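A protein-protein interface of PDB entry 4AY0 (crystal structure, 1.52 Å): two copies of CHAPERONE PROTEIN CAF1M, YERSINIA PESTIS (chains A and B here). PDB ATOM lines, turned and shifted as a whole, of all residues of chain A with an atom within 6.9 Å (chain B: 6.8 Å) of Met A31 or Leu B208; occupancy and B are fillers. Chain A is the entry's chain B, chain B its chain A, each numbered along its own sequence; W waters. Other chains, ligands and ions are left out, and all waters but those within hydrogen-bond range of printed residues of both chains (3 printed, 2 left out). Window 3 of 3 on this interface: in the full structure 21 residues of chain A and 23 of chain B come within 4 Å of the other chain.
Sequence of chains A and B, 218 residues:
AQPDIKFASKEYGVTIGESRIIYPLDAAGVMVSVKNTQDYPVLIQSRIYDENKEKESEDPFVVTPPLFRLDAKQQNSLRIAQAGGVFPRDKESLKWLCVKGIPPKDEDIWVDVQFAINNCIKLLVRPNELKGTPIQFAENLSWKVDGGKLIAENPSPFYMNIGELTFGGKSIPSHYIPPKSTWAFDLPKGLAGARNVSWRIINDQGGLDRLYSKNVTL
No position is printed for both chains.
Of the 6 pairs that touch across the chains among the printed residues, none has its exchanged pair printed and touching as well.
N of Gly B163 is in hydrogen-bond range of O of Arg B200 (2.8 Å).
OE1 of Glu B164 is in salt-bridge range of NE of Arg B200, 3.1 Å away.
The backbone carbonyl oxygen (O) of Asp B209 sits at hydrogen-bond distance from the guanidinium group (NH1) of Arg B200, at 3.0 Å.
Of the 13 printed residues of chain A, 3 touch a printed residue of chain B.
Hydrophobic or aromatic side chains of chain A within 4 Å of the printed part of chain B: Met A31.
Printed residues of chain B that touch a printed residue of chain A: Gly B17, Glu B164, Arg B200 and Leu B208.
Among the printed residues, 6 pairs touch across the chains.
Water W3 lies within hydrogen-bond range of the backbone carbonyl oxygen of Gly B163 and the side-chain hydroxyl of Ser A33.
Water W2 bridges O of Leu B208 (2.7 Å) and N of Met A31 (2.8 Å).
Water W1 lies within hydrogen-bond range of N of Ser A33 (2.8 Å) and N of Leu B208 (3.5 Å).
The backbone NH (N) of Gly B17 sits at hydrogen-bond distance from the backbone carbonyl oxygen (O) of Ser A33, at 2.8 Å.
Among the printed residues, pairs that only touch across the chains: Met A31 with Arg B200 (3.7 Å), Met A31 with Leu B208 (3.6 Å), Ser A33 with Leu B208 (3.9 Å), Ser A77 with Glu B164 (3.96 Å) and Ser A77 with Leu B208 (3.4 Å).
Of the printed residues of chain A, Leu B208 touches Met A31, Ser A33 and Ser A77.
Of the printed residues of chain B, Ser A33 touches Gly B17 and Leu B208.
Of the printed residues of chain B, Ser A77 touches Glu B164 and Leu B208.
Of the printed residues of chain A, Arg B200 touches Met A31 (3.7 Å).
Of the printed residues of chain A, Glu B164 touches Ser A77 (3.96 Å).
Ile B201 touches none of the printed residues of chain A.
The nearest residue of chain B that does not touch Met A31 is Gly B207 (4.9 Å).
The nearest printed residue of chain A that does not touch Leu B208 is Val A32 (4.1 Å).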
ATOM      1  N   ILE A  21     -24.323 -12.925  -7.614  1.00  0.00           N
ATOM      2  CA  ILE A  21     -23.862 -11.570  -7.890  1.00  0.00           C
ATOM      3  C   ILE A  21     -23.340 -11.570  -9.313  1.00  0.00           C
ATOM      4  O   ILE A  21     -22.472 -12.378  -9.657  1.00  0.00           O
ATOM      5  CB  ILE A  21     -22.721 -11.149  -6.930  1.00  0.00           C
ATOM      6  CG1 ILE A  21     -23.211 -11.229  -5.478  1.00  0.00           C
ATOM      7  CG2 ILE A  21     -22.226  -9.742  -7.263  1.00  0.00           C
ATOM      8  CD1 ILE A  21     -22.099 -11.121  -4.432  1.00  0.00           C
ATOM      9  N   GLY A  29     -16.340  -1.517  -9.428  1.00  0.00           N
ATOM     10  CA  GLY A  29     -16.828  -2.313  -8.315  1.00  0.00           C
ATOM     11  C   GLY A  29     -18.332  -2.484  -8.297  1.00  0.00           C
ATOM     12  O   GLY A  29     -19.047  -1.911  -9.128  1.00  0.00           O
ATOM     13  N   VAL A  30     -18.813  -3.300  -7.358  1.00  0.00           N
ATOM     14  CA  VAL A  30     -20.245  -3.420  -7.088  1.00  0.00           C
ATOM     15  C   VAL A  30     -20.442  -3.395  -5.578  1.00  0.00           C
ATOM     16  O   VAL A  30     -19.534  -3.745  -4.823  1.00  0.00           O
ATOM     17  CB  VAL A  30     -20.859  -4.725  -7.653  1.00  0.00           C
ATOM     18  CG1 VAL A  30     -20.659  -4.830  -9.163  1.00  0.00           C
ATOM     19  CG2 VAL A  30     -20.288  -5.954  -6.946  1.00  0.00           C
ATOM     20  N   MET A  31     -21.614  -2.959  -5.134  1.00  0.00           N
ATOM     21  CA  MET A  31     -21.968  -3.030  -3.714  1.00  0.00           C
ATOM     22  C   MET A  31     -22.900  -4.212  -3.458  1.00  0.00           C
ATOM     23  O   MET A  31     -23.757  -4.553  -4.286  1.00  0.00           O
ATOM     24  CB  MET A  31     -22.622  -1.727  -3.229  1.00  0.00           C
ATOM     25  CG  MET A  31     -21.761  -0.457  -3.371  1.00  0.00           C
ATOM     26  SD  MET A  31     -20.194  -0.518  -2.455  1.00  0.00           S
ATOM     27  CE  MET A  31     -20.755  -0.490  -0.759  1.00  0.00           C
ATOM     28  N   VAL A  32     -22.726  -4.842  -2.297  1.00  0.00           N
ATOM     29  CA  VAL A  32     -23.497  -6.021  -1.914  1.00  0.00           C
ATOM     30  C   VAL A  32     -23.958  -5.888  -0.462  1.00  0.00           C
ATOM     31  O   VAL A  32     -23.160  -5.556   0.411  1.00  0.00           O
ATOM     32  CB  VAL A  32     -22.637  -7.305  -2.054  1.00  0.00           C
ATOM     33  CG1 VAL A  32     -23.357  -8.503  -1.489  1.00  0.00           C
ATOM     34  CG2 VAL A  32     -22.302  -7.553  -3.507  1.00  0.00           C
ATOM     35  N   SER A  33     -25.239  -6.150  -0.206  1.00  0.00           N
ATOM     36  CA  SER A  33     -25.779  -6.062   1.151  1.00  0.00           C
ATOM     37  C   SER A  33     -25.643  -7.372   1.932  1.00  0.00           C
ATOM     38  O   SER A  33     -25.888  -8.459   1.401  1.00  0.00           O
ATOM     39  CB  SER A  33     -27.241  -5.613   1.125  1.00  0.00           C
ATOM     40  OG  SER A  33     -27.737  -5.419   2.438  1.00  0.00           O
ATOM     41  N   VAL A  34     -25.221  -7.266   3.188  1.00  0.00           N
ATOM     42  CA  VAL A  34     -25.197  -8.425   4.083  1.00  0.00           C
ATOM     43  C   VAL A  34     -26.052  -8.124   5.307  1.00  0.00           C
ATOM     44  O   VAL A  34     -26.106  -6.988   5.781  1.00  0.00           O
ATOM     45  CB  VAL A  34     -23.763  -8.856   4.502  1.00  0.00           C
ATOM     46  CG1 VAL A  34     -22.951  -9.288   3.291  1.00  0.00           C
ATOM     47  CG2 VAL A  34     -23.049  -7.743   5.255  1.00  0.00           C
ATOM     48  N   THR A  64     -14.304  -4.757   0.823  1.00  0.00           N
ATOM     49  CA  THR A  64     -14.156  -3.733   1.851  1.00  0.00           C
ATOM     50  C   THR A  64     -15.507  -3.448   2.481  1.00  0.00           C
ATOM     51  O   THR A  64     -16.476  -3.135   1.783  1.00  0.00           O
ATOM     52  CB  THR A  64     -13.585  -2.440   1.264  1.00  0.00           C
ATOM     53  OG1 THR A  64     -12.458  -2.755   0.437  1.00  0.00           O
ATOM     54  CG2 THR A  64     -13.131  -1.500   2.381  1.00  0.00           C
ATOM     55  N   ASN A  76     -25.480  -4.306   6.438  1.00  0.00           N
ATOM     56  CA  ASN A  76     -24.327  -3.519   6.007  1.00  0.00           C
ATOM     57  C   ASN A  76     -23.974  -3.798   4.553  1.00  0.00           C
ATOM     58  O   ASN A  76     -24.192  -4.896   4.050  1.00  0.00           O
ATOM     59  CB  ASN A  76     -23.109  -3.824   6.890  1.00  0.00           C
ATOM     60  CG  ASN A  76     -22.132  -2.673   6.958  1.00  0.00           C
ATOM     61  OD1 ASN A  76     -21.101  -2.664   6.273  1.00  0.00           O
ATOM     62  ND2 ASN A  76     -22.445  -1.696   7.792  1.00  0.00           N
ATOM     63  N   SER A  77     -23.403  -2.811   3.879  1.00  0.00           N
ATOM     64  CA  SER A  77     -22.963  -3.011   2.510  1.00  0.00           C
ATOM     65  C   SER A  77     -21.469  -3.338   2.427  1.00  0.00           C
ATOM     66  O   SER A  77     -20.668  -2.786   3.184  1.00  0.00           O
ATOM     67  CB  SER A  77     -23.279  -1.764   1.679  1.00  0.00           C
ATOM     68  OG  SER A  77     -24.676  -1.519   1.664  1.00  0.00           O
ATOM     69  N   LEU A  78     -21.121  -4.243   1.516  1.00  0.00           N
ATOM     70  CA  LEU A  78     -19.726  -4.549   1.185  1.00  0.00           C
ATOM     71  C   LEU A  78     -19.425  -4.013  -0.204  1.00  0.00           C
ATOM     72  O   LEU A  78     -20.260  -4.107  -1.104  1.00  0.00           O
ATOM     73  CB  LEU A  78     -19.499  -6.061   1.128  1.00  0.00           C
ATOM     74  CG  LEU A  78     -19.890  -6.989   2.276  1.00  0.00           C
ATOM     75  CD1 LEU A  78     -19.686  -8.433   1.854  1.00  0.00           C
ATOM     76  CD2 LEU A  78     -19.074  -6.683   3.509  1.00  0.00           C
ATOM     77  N   ARG A  79     -18.224  -3.481  -0.394  1.00  0.00           N
ATOM     78  CA  ARG A  79     -17.764  -3.166  -1.737  1.00  0.00           C
ATOM     79  C   ARG A  79     -16.935  -4.332  -2.267  1.00  0.00           C
ATOM     80  O   ARG A  79     -16.016  -4.800  -1.590  1.00  0.00           O
ATOM     81  CB  ARG A  79     -16.943  -1.884  -1.739  1.00  0.00           C
ATOM     82  CG  ARG A  79     -16.345  -1.549  -3.090  1.00  0.00           C
ATOM     83  CD  ARG A  79     -15.768  -0.151  -3.091  1.00  0.00           C
ATOM     84  NE  ARG A  79     -15.090   0.161  -4.346  1.00  0.00           N
ATOM     85  CZ  ARG A  79     -15.718   0.547  -5.450  1.00  0.00           C
ATOM     86  NH1 ARG A  79     -17.041   0.655  -5.453  1.00  0.00           N
ATOM     87  NH2 ARG A  79     -15.024   0.822  -6.550  1.00  0.00           N
ATOM     88  N   ILE A  80     -17.274  -4.809  -3.459  1.00  0.00           N
ATOM     89  CA  ILE A  80     -16.453  -5.805  -4.159  1.00  0.00           C
ATOM     90  C   ILE A  80     -15.818  -5.137  -5.366  1.00  0.00           C
ATOM     91  O   ILE A  80     -16.528  -4.676  -6.263  1.00  0.00           O
ATOM     92  CB  ILE A  80     -17.285  -7.021  -4.633  1.00  0.00           C
ATOM     93  CG1 ILE A  80     -17.994  -7.681  -3.447  1.00  0.00           C
ATOM     94  CG2 ILE A  80     -16.399  -8.035  -5.345  1.00  0.00           C
ATOM     95  CD1 ILE A  80     -18.902  -8.816  -3.855  1.00  0.00           C
ATOM     96  N   GLY B  17     -27.284 -10.299  -0.207  1.00  0.00           N
ATOM     97  CA  GLY B  17     -28.277  -9.852  -1.176  1.00  0.00           C
ATOM     98  C   GLY B  17     -29.693 -10.093  -0.694  1.00  0.00           C
ATOM     99  O   GLY B  17     -29.920 -10.444   0.466  1.00  0.00           O
ATOM    100  N   ASN B 161     -37.527  -0.582  -5.088  1.00  0.00           N
ATOM    101  CA  ASN B 161     -37.256  -1.224  -3.818  1.00  0.00           C
ATOM    102  C   ASN B 161     -35.957  -0.683  -3.236  1.00  0.00           C
ATOM    103  O   ASN B 161     -34.878  -1.072  -3.638  1.00  0.00           O
ATOM    104  CB  ASN B 161     -37.224  -2.747  -4.003  1.00  0.00           C
ATOM    105  CG  ASN B 161     -38.578  -3.298  -4.423  1.00  0.00           C
ATOM    106  OD1 ASN B 161     -39.552  -3.161  -3.685  1.00  0.00           O
ATOM    107  ND2 ASN B 161     -38.655  -3.898  -5.607  1.00  0.00           N
ATOM    108  N   ILE B 162     -36.076   0.256  -2.311  1.00  0.00           N
ATOM    109  CA  ILE B 162     -34.898   0.906  -1.742  1.00  0.00           C
ATOM    110  C   ILE B 162     -34.008  -0.077  -0.968  1.00  0.00           C
ATOM    111  O   ILE B 162     -34.492  -0.864  -0.141  1.00  0.00           O
ATOM    112  CB  ILE B 162     -35.335   2.043  -0.812  1.00  0.00           C
ATOM    113  CG1 ILE B 162     -36.120   3.090  -1.598  1.00  0.00           C
ATOM    114  CG2 ILE B 162     -34.143   2.648  -0.090  1.00  0.00           C
ATOM    115  CD1 ILE B 162     -35.301   3.873  -2.596  1.00  0.00           C
ATOM    116  N   GLY B 163     -32.706  -0.041  -1.249  1.00  0.00           N
ATOM    117  CA  GLY B 163     -31.723  -0.832  -0.519  1.00  0.00           C
ATOM    118  C   GLY B 163     -30.831   0.012   0.379  1.00  0.00           C
ATOM    119  O   GLY B 163     -30.273  -0.477   1.358  1.00  0.00           O
ATOM    120  N   GLU B 164     -30.718   1.298   0.063  1.00  0.00           N
ATOM    121  CA  GLU B 164     -29.907   2.214   0.852  1.00  0.00           C
ATOM    122  C   GLU B 164     -30.534   3.585   0.711  1.00  0.00           C
ATOM    123  O   GLU B 164     -30.880   3.989  -0.395  1.00  0.00           O
ATOM    124  CB  GLU B 164     -28.476   2.241   0.318  1.00  0.00           C
ATOM    125  CG  GLU B 164     -27.541   3.211   1.008  1.00  0.00           C
ATOM    126  CD  GLU B 164     -26.147   3.180   0.406  1.00  0.00           C
ATOM    127  OE1 GLU B 164     -25.590   2.068   0.255  1.00  0.00           O
ATOM    128  OE2 GLU B 164     -25.617   4.262   0.074  1.00  0.00           O
ATOM    129  N   ARG B 200     -29.961   3.999  -3.161  1.00  0.00           N
ATOM    130  CA  ARG B 200     -29.724   2.907  -4.107  1.00  0.00           C
ATOM    131  C   ARG B 200     -30.975   2.059  -4.112  1.00  0.00           C
ATOM    132  O   ARG B 200     -31.507   1.740  -3.048  1.00  0.00           O
ATOM    133  CB  ARG B 200     -28.561   2.005  -3.667  1.00  0.00           C
ATOM    134  CG  ARG B 200     -27.223   2.689  -3.518  1.00  0.00           C
ATOM    135  CD  ARG B 200     -26.185   1.675  -3.019  1.00  0.00           C
ATOM    136  NE  ARG B 200     -24.911   2.320  -2.740  1.00  0.00           N
ATOM    137  CZ  ARG B 200     -23.953   2.475  -3.642  1.00  0.00           C
ATOM    138  NH1 ARG B 200     -24.123   1.985  -4.863  1.00  0.00           N
ATOM    139  NH2 ARG B 200     -22.830   3.099  -3.319  1.00  0.00           N
ATOM    140  N   ILE B 201     -31.457   1.670  -5.287  1.00  0.00           N
ATOM    141  CA  ILE B 201     -32.485   0.625  -5.329  1.00  0.00           C
ATOM    142  C   ILE B 201     -31.830  -0.751  -5.344  1.00  0.00           C
ATOM    143  O   ILE B 201     -30.609  -0.877  -5.526  1.00  0.00           O
ATOM    144  CB  ILE B 201     -33.461   0.770  -6.526  1.00  0.00           C
ATOM    145  CG1 ILE B 201     -32.778   0.442  -7.867  1.00  0.00           C
ATOM    146  CG2 ILE B 201     -34.091   2.160  -6.546  1.00  0.00           C
ATOM    147  CD1 ILE B 201     -33.779   0.084  -8.985  1.00  0.00           C
ATOM    148  N   ILE B 202     -32.652  -1.776  -5.133  1.00  0.00           N
ATOM    149  CA  ILE B 202     -32.250  -3.175  -5.304  1.00  0.00           C
ATOM    150  C   ILE B 202     -32.740  -3.576  -6.686  1.00  0.00           C
ATOM    151  O   ILE B 202     -33.904  -3.350  -7.032  1.00  0.00           O
ATOM    152  CB  ILE B 202     -32.883  -4.071  -4.218  1.00  0.00           C
ATOM    153  CG1 ILE B 202     -32.386  -3.630  -2.831  1.00  0.00           C
ATOM    154  CG2 ILE B 202     -32.583  -5.542  -4.479  1.00  0.00           C
ATOM    155  CD1 ILE B 202     -33.178  -4.204  -1.665  1.00  0.00           C
ATOM    156  N   ASN B 203     -31.840  -4.130  -7.498  1.00  0.00           N
ATOM    157  CA  ASN B 203     -32.190  -4.548  -8.853  1.00  0.00           C
ATOM    158  C   ASN B 203     -32.942  -5.889  -8.860  1.00  0.00           C
ATOM    159  O   ASN B 203     -33.141  -6.514  -7.801  1.00  0.00           O
ATOM    160  CB  ASN B 203     -30.933  -4.577  -9.746  1.00  0.00           C
ATOM    161  CG  ASN B 203     -29.868  -5.540  -9.235  1.00  0.00           C
ATOM    162  OD1 ASN B 203     -30.176  -6.645  -8.781  1.00  0.00           O
ATOM    163  ND2 ASN B 203     -28.602  -5.121  -9.308  1.00  0.00           N
ATOM    164  N   GLY B 206     -31.491  -8.851  -7.035  1.00  0.00           N
ATOM    165  CA  GLY B 206     -31.338  -8.821  -5.592  1.00  0.00           C
ATOM    166  C   GLY B 206     -30.107  -8.076  -5.109  1.00  0.00           C
ATOM    167  O   GLY B 206     -29.782  -8.107  -3.919  1.00  0.00           O
ATOM    168  N   GLY B 207     -29.441  -7.382  -6.022  1.00  0.00           N
ATOM    169  CA  GLY B 207     -28.218  -6.672  -5.689  1.00  0.00           C
ATOM    170  C   GLY B 207     -28.424  -5.175  -5.575  1.00  0.00           C
ATOM    171  O   GLY B 207     -29.421  -4.644  -6.047  1.00  0.00           O
ATOM    172  N   LEU B 208     -27.477  -4.490  -4.944  1.00  0.00           N
ATOM    173  CA  LEU B 208     -27.571  -3.039  -4.830  1.00  0.00           C
ATOM    174  C   LEU B 208     -27.177  -2.364  -6.139  1.00  0.00           C
ATOM    175  O   LEU B 208     -26.141  -2.689  -6.739  1.00  0.00           O
ATOM    176  CB  LEU B 208     -26.690  -2.528  -3.687  1.00  0.00           C
ATOM    177  CG  LEU B 208     -27.135  -2.891  -2.275  1.00  0.00           C
ATOM    178  CD1 LEU B 208     -26.050  -2.492  -1.282  1.00  0.00           C
ATOM    179  CD2 LEU B 208     -28.431  -2.158  -1.954  1.00  0.00           C
ATOM    180  N   ASP B 209     -27.988  -1.399  -6.560  1.00  0.00           N
ATOM    181  CA  ASP B 209     -27.747  -0.622  -7.776  1.00  0.00           C
ATOM    182  C   ASP B 209     -26.865   0.583  -7.444  1.00  0.00           C
ATOM    183  O   ASP B 209     -26.529   0.810  -6.273  1.00  0.00           O
ATOM    184  CB  ASP B 209     -29.100  -0.179  -8.364  1.00  0.00           C
ATOM    185  CG  ASP B 209     -28.975   0.500  -9.728  1.00  0.00           C
ATOM    186  OD1 ASP B 209     -28.118   0.077 -10.539  1.00  0.00           O
ATOM    187  OD2 ASP B 209     -29.753   1.458  -9.983  1.00  0.00           O
ATOM    188  N   ARG B 210     -26.487   1.355  -8.463  1.00  0.00           N
ATOM    189  CA  ARG B 210     -25.647   2.537  -8.263  1.00  0.00           C
ATOM    190  C   ARG B 210     -26.306   3.603  -7.386  1.00  0.00           C
ATOM    191  O   ARG B 210     -27.540   3.658  -7.235  1.00  0.00           O
ATOM    192  CB  ARG B 210     -25.230   3.152  -9.605  1.00  0.00           C
ATOM    193  CG  ARG B 210     -26.389   3.611 -10.476  1.00  0.00           C
ATOM    194  CD  ARG B 210     -25.950   4.714 -11.424  1.00  0.00           C
ATOM    195  NE  ARG B 210     -25.713   5.951 -10.684  1.00  0.00           N
ATOM    196  CZ  ARG B 210     -25.547   7.148 -11.240  1.00  0.00           C
ATOM    197  NH1 ARG B 210     -25.597   7.287 -12.559  1.00  0.00           N
ATOM    198  NH2 ARG B 210     -25.343   8.210 -10.472  1.00  0.00           N
HETATM  199  O   HOH W   1     -26.763  -6.787  -2.459  1.00  0.00           O
HETATM  200  O   HOH W   2     -23.522  -2.060  -7.035  1.00  0.00           O
HETATM  201  O   HOH W   3     -29.823  -3.118   1.470  1.00  0.00           O
